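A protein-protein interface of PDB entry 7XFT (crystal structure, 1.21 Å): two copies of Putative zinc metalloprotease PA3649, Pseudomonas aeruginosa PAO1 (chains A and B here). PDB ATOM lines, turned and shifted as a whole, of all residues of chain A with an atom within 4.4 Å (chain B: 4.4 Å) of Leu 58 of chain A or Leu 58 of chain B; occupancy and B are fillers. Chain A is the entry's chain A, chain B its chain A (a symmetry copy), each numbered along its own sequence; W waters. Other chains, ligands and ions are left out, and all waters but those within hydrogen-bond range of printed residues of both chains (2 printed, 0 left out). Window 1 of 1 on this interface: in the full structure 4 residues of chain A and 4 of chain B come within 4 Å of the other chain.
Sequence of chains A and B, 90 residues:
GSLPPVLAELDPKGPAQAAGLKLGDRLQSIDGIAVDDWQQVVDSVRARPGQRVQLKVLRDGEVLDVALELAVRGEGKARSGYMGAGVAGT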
ATOM      1  N   GLY A  24      -2.367  24.927  23.104  1.00  0.00           N
ATOM      2  CA  GLY A  24      -0.983  24.570  22.920  1.00  0.00           C
ATOM      3  C   GLY A  24      -0.089  24.826  24.107  1.00  0.00           C
ATOM      4  O   GLY A  24       1.053  24.352  24.116  1.00  0.00           O
ATOM      5  N   ASP A  25      -0.544  25.570  25.107  1.00  0.00           N
ATOM      6  CA  ASP A  25       0.281  25.768  26.285  1.00  0.00           C
ATOM      7  C   ASP A  25       0.513  24.434  26.986  1.00  0.00           C
ATOM      8  O   ASP A  25      -0.388  23.595  27.084  1.00  0.00           O
ATOM      9  CB  ASP A  25      -0.412  26.710  27.265  1.00  0.00           C
ATOM     10  CG  ASP A  25      -0.339  28.171  26.866  1.00  0.00           C
ATOM     11  OD1 ASP A  25       0.335  28.543  25.873  1.00  0.00           O
ATOM     12  OD2 ASP A  25      -0.964  28.965  27.600  1.00  0.00           O
ATOM     13  N   ARG A  26       1.728  24.245  27.490  1.00  0.00           N
ATOM     14  CA  ARG A  26       2.133  23.007  28.153  1.00  0.00           C
ATOM     15  C   ARG A  26       2.394  23.323  29.612  1.00  0.00           C
ATOM     16  O   ARG A  26       3.301  24.090  29.933  1.00  0.00           O
ATOM     17  CB  ARG A  26       3.408  22.442  27.515  1.00  0.00           C
ATOM     18  CG  ARG A  26       3.821  21.084  28.021  1.00  0.00           C
ATOM     19  CD  ARG A  26       5.088  20.541  27.316  1.00  0.00           C
ATOM     20  NE  ARG A  26       4.934  20.601  25.864  1.00  0.00           N
ATOM     21  CZ  ARG A  26       4.464  19.624  25.106  1.00  0.00           C
ATOM     22  NH1 ARG A  26       4.333  18.397  25.574  1.00  0.00           N
ATOM     23  NH2 ARG A  26       4.085  19.895  23.855  1.00  0.00           N
ATOM     24  N   GLN A  28       3.896  22.960  33.087  1.00  0.00           N
ATOM     25  CA  GLN A  28       5.091  22.348  33.650  1.00  0.00           C
ATOM     26  C   GLN A  28       4.967  22.066  35.132  1.00  0.00           C
ATOM     27  O   GLN A  28       5.460  21.036  35.599  1.00  0.00           O
ATOM     28  CB  GLN A  28       6.271  23.285  33.442  1.00  0.00           C
ATOM     29  CG  GLN A  28       6.703  23.357  32.017  1.00  0.00           C
ATOM     30  CD  GLN A  28       7.902  24.234  31.855  1.00  0.00           C
ATOM     31  OE1 GLN A  28       8.045  25.249  32.541  1.00  0.00           O
ATOM     32  NE2 GLN A  28       8.804  23.827  30.982  1.00  0.00           N
ATOM     33  N   VAL A  57       4.243  27.516  32.698  1.00  0.00           N
ATOM     34  CA  VAL A  57       3.691  27.064  31.429  1.00  0.00           C
ATOM     35  C   VAL A  57       4.720  27.318  30.339  1.00  0.00           C
ATOM     36  O   VAL A  57       5.349  28.381  30.305  1.00  0.00           O
ATOM     37  CB  VAL A  57       2.399  27.863  31.144  1.00  0.00           C
ATOM     38  CG1 VAL A  57       1.887  27.690  29.746  1.00  0.00           C
ATOM     39  CG2 VAL A  57       1.324  27.529  32.183  1.00  0.00           C
ATOM     40  N   LEU A  58       4.853  26.373  29.415  1.00  0.00           N
ATOM     41  CA  LEU A  58       5.703  26.554  28.250  1.00  0.00           C
ATOM     42  C   LEU A  58       4.835  26.935  27.064  1.00  0.00           C
ATOM     43  O   LEU A  58       3.879  26.221  26.727  1.00  0.00           O
ATOM     44  CB  LEU A  58       6.431  25.253  27.953  1.00  0.00           C
ATOM     45  CG  LEU A  58       7.419  25.249  26.805  1.00  0.00           C
ATOM     46  CD1 LEU A  58       8.576  26.181  27.064  1.00  0.00           C
ATOM     47  CD2 LEU A  58       7.954  23.838  26.652  1.00  0.00           C
ATOM     48  N   ARG A  59       5.193  28.043  26.423  1.00  0.00           N
ATOM     49  CA  ARG A  59       4.507  28.537  25.235  1.00  0.00           C
ATOM     50  C   ARG A  59       5.561  28.895  24.198  1.00  0.00           C
ATOM     51  O   ARG A  59       6.319  29.853  24.385  1.00  0.00           O
ATOM     52  CB  ARG A  59       3.650  29.760  25.571  1.00  0.00           C
ATOM     53  CG  ARG A  59       2.868  30.274  24.356  1.00  0.00           C
ATOM     54  CD  ARG A  59       2.064  31.521  24.656  1.00  0.00           C
ATOM     55  NE  ARG A  59       1.073  31.228  25.675  1.00  0.00           N
ATOM     56  CZ  ARG A  59       0.607  32.107  26.545  1.00  0.00           C
ATOM     57  NH1 ARG A  59       0.933  33.388  26.479  1.00  0.00           N
ATOM     58  NH2 ARG A  59      -0.199  31.687  27.505  1.00  0.00           N
ATOM     59  N   ASP A  60       5.612  28.127  23.117  1.00  0.00           N
ATOM     60  CA  ASP A  60       6.498  28.421  21.995  1.00  0.00           C
ATOM     61  C   ASP A  60       7.914  28.756  22.451  1.00  0.00           C
ATOM     62  O   ASP A  60       8.489  29.770  22.062  1.00  0.00           O
ATOM     63  CB  ASP A  60       5.926  29.549  21.136  1.00  0.00           C
ATOM     64  CG  ASP A  60       6.680  29.732  19.825  1.00  0.00           C
ATOM     65  OD1 ASP A  60       7.151  28.726  19.247  1.00  0.00           O
ATOM     66  OD2 ASP A  60       6.800  30.884  19.376  1.00  0.00           O
ATOM     67  N   GLY A  61       8.472  27.892  23.300  1.00  0.00           N
ATOM     68  CA  GLY A  61       9.853  28.012  23.722  1.00  0.00           C
ATOM     69  C   GLY A  61      10.101  28.924  24.903  1.00  0.00           C
ATOM     70  O   GLY A  61      11.253  29.043  25.335  1.00  0.00           O
ATOM     71  N   GLU A  62       9.071  29.557  25.456  1.00  0.00           N
ATOM     72  CA  GLU A  62       9.236  30.469  26.575  1.00  0.00           C
ATOM     73  C   GLU A  62       8.478  29.937  27.785  1.00  0.00           C
ATOM     74  O   GLU A  62       7.317  29.525  27.675  1.00  0.00           O
ATOM     75  CB  GLU A  62       8.706  31.853  26.203  1.00  0.00           C
ATOM     76  CG  GLU A  62       8.918  32.923  27.230  1.00  0.00           C
ATOM     77  CD  GLU A  62       8.651  34.337  26.681  1.00  0.00           C
ATOM     78  OE1 GLU A  62       8.474  34.528  25.432  1.00  0.00           O
ATOM     79  OE2 GLU A  62       8.645  35.276  27.535  1.00  0.00           O
ATOM     80  N   VAL A  63       9.133  29.962  28.937  1.00  0.00           N
ATOM     81  CA  VAL A  63       8.523  29.556  30.199  1.00  0.00           C
ATOM     82  C   VAL A  63       7.842  30.762  30.824  1.00  0.00           C
ATOM     83  O   VAL A  63       8.480  31.796  31.064  1.00  0.00           O
ATOM     84  CB  VAL A  63       9.582  28.988  31.150  1.00  0.00           C
ATOM     85  CG1 VAL A  63       8.969  28.670  32.513  1.00  0.00           C
ATOM     86  CG2 VAL A  63      10.210  27.757  30.563  1.00  0.00           C
ATOM     87  N   GLY B  24      17.502  24.889  20.173  1.00  0.00           N
ATOM     88  CA  GLY B  24      16.165  25.068  20.682  1.00  0.00           C
ATOM     89  C   GLY B  24      15.532  23.835  21.274  1.00  0.00           C
ATOM     90  O   GLY B  24      14.486  23.946  21.925  1.00  0.00           O
ATOM     91  N   ASP B  25      16.103  22.655  21.067  1.00  0.00           N
ATOM     92  CA  ASP B  25      15.542  21.468  21.687  1.00  0.00           C
ATOM     93  C   ASP B  25      15.634  21.584  23.205  1.00  0.00           C
ATOM     94  O   ASP B  25      16.630  22.068  23.752  1.00  0.00           O
ATOM     95  CB  ASP B  25      16.314  20.227  21.254  1.00  0.00           C
ATOM     96  CG  ASP B  25      15.978  19.755  19.852  1.00  0.00           C
ATOM     97  OD1 ASP B  25      15.061  20.295  19.184  1.00  0.00           O
ATOM     98  OD2 ASP B  25      16.649  18.790  19.430  1.00  0.00           O
ATOM     99  N   ARG B  26      14.594  21.120  23.889  1.00  0.00           N
ATOM    100  CA  ARG B  26      14.499  21.194  25.345  1.00  0.00           C
ATOM    101  C   ARG B  26      14.531  19.779  25.887  1.00  0.00           C
ATOM    102  O   ARG B  26      13.632  18.985  25.615  1.00  0.00           O
ATOM    103  CB  ARG B  26      13.193  21.875  25.770  1.00  0.00           C
ATOM    104  CG  ARG B  26      13.070  22.144  27.249  1.00  0.00           C
ATOM    105  CD  ARG B  26      11.755  22.871  27.620  1.00  0.00           C
ATOM    106  NE  ARG B  26      11.575  24.063  26.793  1.00  0.00           N
ATOM    107  CZ  ARG B  26      11.981  25.280  27.112  1.00  0.00           C
ATOM    108  NH1 ARG B  26      12.360  25.575  28.341  1.00  0.00           N
ATOM    109  NH2 ARG B  26      12.038  26.217  26.164  1.00  0.00           N
ATOM    110  N   GLN B  28      13.891  16.909  28.298  1.00  0.00           N
ATOM    111  CA  GLN B  28      12.934  16.628  29.358  1.00  0.00           C
ATOM    112  C   GLN B  28      13.417  15.566  30.324  1.00  0.00           C
ATOM    113  O   GLN B  28      13.168  15.679  31.527  1.00  0.00           O
ATOM    114  CB  GLN B  28      11.633  16.148  28.735  1.00  0.00           C
ATOM    115  CG  GLN B  28      10.890  17.239  28.043  1.00  0.00           C
ATOM    116  CD  GLN B  28       9.587  16.751  27.497  1.00  0.00           C
ATOM    117  OE1 GLN B  28       9.477  15.612  27.037  1.00  0.00           O
ATOM    118  NE2 GLN B  28       8.571  17.588  27.588  1.00  0.00           N
ATOM    119  N   VAL B  57      12.915  14.711  24.394  1.00  0.00           N
ATOM    120  CA  VAL B  57      13.223  16.078  23.997  1.00  0.00           C
ATOM    121  C   VAL B  57      11.955  16.720  23.457  1.00  0.00           C
ATOM    122  O   VAL B  57      11.210  16.094  22.696  1.00  0.00           O
ATOM    123  CB  VAL B  57      14.313  16.037  22.902  1.00  0.00           C
ATOM    124  CG1 VAL B  57      14.520  17.354  22.217  1.00  0.00           C
ATOM    125  CG2 VAL B  57      15.624  15.487  23.473  1.00  0.00           C
ATOM    126  N   LEU B  58      11.737  17.985  23.798  1.00  0.00           N
ATOM    127  CA  LEU B  58      10.635  18.751  23.240  1.00  0.00           C
ATOM    128  C   LEU B  58      11.166  19.634  22.126  1.00  0.00           C
ATOM    129  O   LEU B  58      12.103  20.418  22.334  1.00  0.00           O
ATOM    130  CB  LEU B  58      10.023  19.616  24.330  1.00  0.00           C
ATOM    131  CG  LEU B  58       8.814  20.451  23.965  1.00  0.00           C
ATOM    132  CD1 LEU B  58       7.638  19.589  23.580  1.00  0.00           C
ATOM    133  CD2 LEU B  58       8.433  21.281  25.177  1.00  0.00           C
ATOM    134  N   ARG B  59      10.543  19.519  20.957  1.00  0.00           N
ATOM    135  CA  ARG B  59      10.884  20.320  19.787  1.00  0.00           C
ATOM    136  C   ARG B  59       9.591  20.859  19.193  1.00  0.00           C
ATOM    137  O   ARG B  59       8.782  20.090  18.660  1.00  0.00           O
ATOM    138  CB  ARG B  59      11.638  19.481  18.754  1.00  0.00           C
ATOM    139  CG  ARG B  59      12.063  20.305  17.532  1.00  0.00           C
ATOM    140  CD  ARG B  59      12.756  19.476  16.472  1.00  0.00           C
ATOM    141  NE  ARG B  59      13.976  18.910  17.018  1.00  0.00           N
ATOM    142  CZ  ARG B  59      14.513  17.766  16.629  1.00  0.00           C
ATOM    143  NH1 ARG B  59      14.027  17.084  15.605  1.00  0.00           N
ATOM    144  NH2 ARG B  59      15.556  17.295  17.291  1.00  0.00           N
ATOM    145  N   ASP B  60       9.395  22.168  19.289  1.00  0.00           N
ATOM    146  CA  ASP B  60       8.254  22.832  18.667  1.00  0.00           C
ATOM    147  C   ASP B  60       6.944  22.098  18.936  1.00  0.00           C
ATOM    148  O   ASP B  60       6.178  21.800  18.022  1.00  0.00           O
ATOM    149  CB  ASP B  60       8.480  23.001  17.165  1.00  0.00           C
ATOM    150  CG  ASP B  60       7.438  23.899  16.510  1.00  0.00           C
ATOM    151  OD1 ASP B  60       6.977  24.868  17.153  1.00  0.00           O
ATOM    152  OD2 ASP B  60       7.082  23.630  15.350  1.00  0.00           O
ATOM    153  N   GLY B  61       6.697  21.796  20.211  1.00  0.00           N
ATOM    154  CA  GLY B  61       5.440  21.212  20.633  1.00  0.00           C
ATOM    155  C   GLY B  61       5.350  19.706  20.535  1.00  0.00           C
ATOM    156  O   GLY B  61       4.317  19.142  20.911  1.00  0.00           O
ATOM    157  N   GLU B  62       6.392  19.028  20.064  1.00  0.00           N
ATOM    158  CA  GLU B  62       6.370  17.582  19.915  1.00  0.00           C
ATOM    159  C   GLU B  62       7.435  16.959  20.808  1.00  0.00           C
ATOM    160  O   GLU B  62       8.585  17.416  20.837  1.00  0.00           O
ATOM    161  CB  GLU B  62       6.631  17.203  18.459  1.00  0.00           C
ATOM    162  CG  GLU B  62       6.524  15.743  18.142  1.00  0.00           C
ATOM    163  CD  GLU B  62       6.488  15.462  16.627  1.00  0.00           C
ATOM    164  OE1 GLU B  62       6.360  16.417  15.792  1.00  0.00           O
ATOM    165  OE2 GLU B  62       6.569  14.242  16.284  1.00  0.00           O
ATOM    166  N   VAL B  63       7.053  15.909  21.522  1.00  0.00           N
ATOM    167  CA  VAL B  63       7.973  15.157  22.369  1.00  0.00           C
ATOM    168  C   VAL B  63       8.623  14.064  21.536  1.00  0.00           C
ATOM    169  O   VAL B  63       7.933  13.225  20.941  1.00  0.00           O
ATOM    170  CB  VAL B  63       7.227  14.546  23.561  1.00  0.00           C
ATOM    171  CG1 VAL B  63       8.161  13.662  24.387  1.00  0.00           C
ATOM    172  CG2 VAL B  63       6.639  15.627  24.422  1.00  0.00           C
HETATM  173  O   HOH W   1      13.305  28.231  27.952  1.00  0.00           O
HETATM  174  O   HOH W   2       3.009  17.161  23.378  1.00  0.00           O
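O of Gly 61 of chain B is in hydrogen-bond range of NH2 of Arg 26 of chain A (3.0 Å).
The guanidinium group (NH2) of Arg 26 of chain B lies within hydrogen-bond range of the backbone carbonyl oxygen (O) of Gly 61 of chain A, at 3.0 Å.
The backbone NH (N) of Leu 58 of chain A sits at hydrogen-bond distance from the backbone carbonyl oxygen (O) of Arg 26 of chain A, 2.8 Å away.
The backbone NH (N) of Leu 58 of chain B lies within hydrogen-bond range of the backbone carbonyl oxygen (O) of Arg 26 of chain B, 2.8 Å away.
Among the printed residues, merely in contact across the chains: Arg 26 of chain A with Leu 58 of chain B (3.5 Å), Arg 26 of chain A with Val 63 of chain B (3.8 Å), Leu 58 of chain A with Arg 26 of chain B (3.5 Å), Leu 58 of chain A with Leu 58 of chain B (3.0 Å) and Val 63 of chain A with Arg 26 of chain B (3.8 Å).
Leu 58 of chain A touches just these residues of chain B: Arg 26 and Leu 58.
Of the printed residues of chain A, Leu 58 of chain B touches Arg 26 and Leu 58.
Of the printed residues of chain B, Gly 61 of chain A touches Arg 26.
Printed residues of chain A within 4 Å of Gly 61 of chain B: Arg 26.
Printed residues of chain A within 4 Å of Arg 26 of chain B: Leu 58 (3.5 Å), Gly 61 (3.0 Å) and Val 63 (3.8 Å).
Of the printed residues of chain B, Arg 26 of chain A touches Leu 58, Gly 61 and Val 63.
Gly 24 of chain A touches none of the printed residues of chain B.
The nearest printed residue of chain B that does not touch Leu 58 of chain A is Gln 28 of chain B (6.3 Å).
The nearest printed residue of chain A that does not touch Leu 58 of chain B is Gln 28 of chain A (6.3 Å).
The nearest printed residue of chain A that does not touch Val 63 of chain B is Leu 58 of chain A (8.6 Å).
Hydrophobic or aromatic side chains of chain A within 4 Å of the printed part of chain B: Leu 58 and Val 63.
Along chain B the printed residues that touch a printed residue of chain A span positions 26 to 63.
Among the printed residues, 7 pairs touch across the chains.
Arg 26 of chain A touches Leu 58 of chain B, and with the chains exchanged Leu 58 of chain A touches Arg 26 of chain B.
Arg 26 of chain A touches Gly 61 of chain B, and with the chains exchanged Gly 61 of chain A touches Arg 26 of chain B.
Arg 26 of chain A touches Val 63 of chain B, and with the chains exchanged Val 63 of chain A touches Arg 26 of chain B.
Leu 58 of chain B touches its own counterpart, Leu 58 of chain A.
Positions printed for both chains: 24, 25, 26, 28, 57, 58, 59, 60, 61, 62 and 63.
Water W1 bridges NH1 of Arg 26 of chain B (2.8 Å) and O of Gly 61 of chain A (3.4 Å).
Water W2 lies within hydrogen-bond range of the guanidinium group (NH1) of Arg 26 of chain A and the backbone carbonyl oxygen (O) of Gly 61 of chain B.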
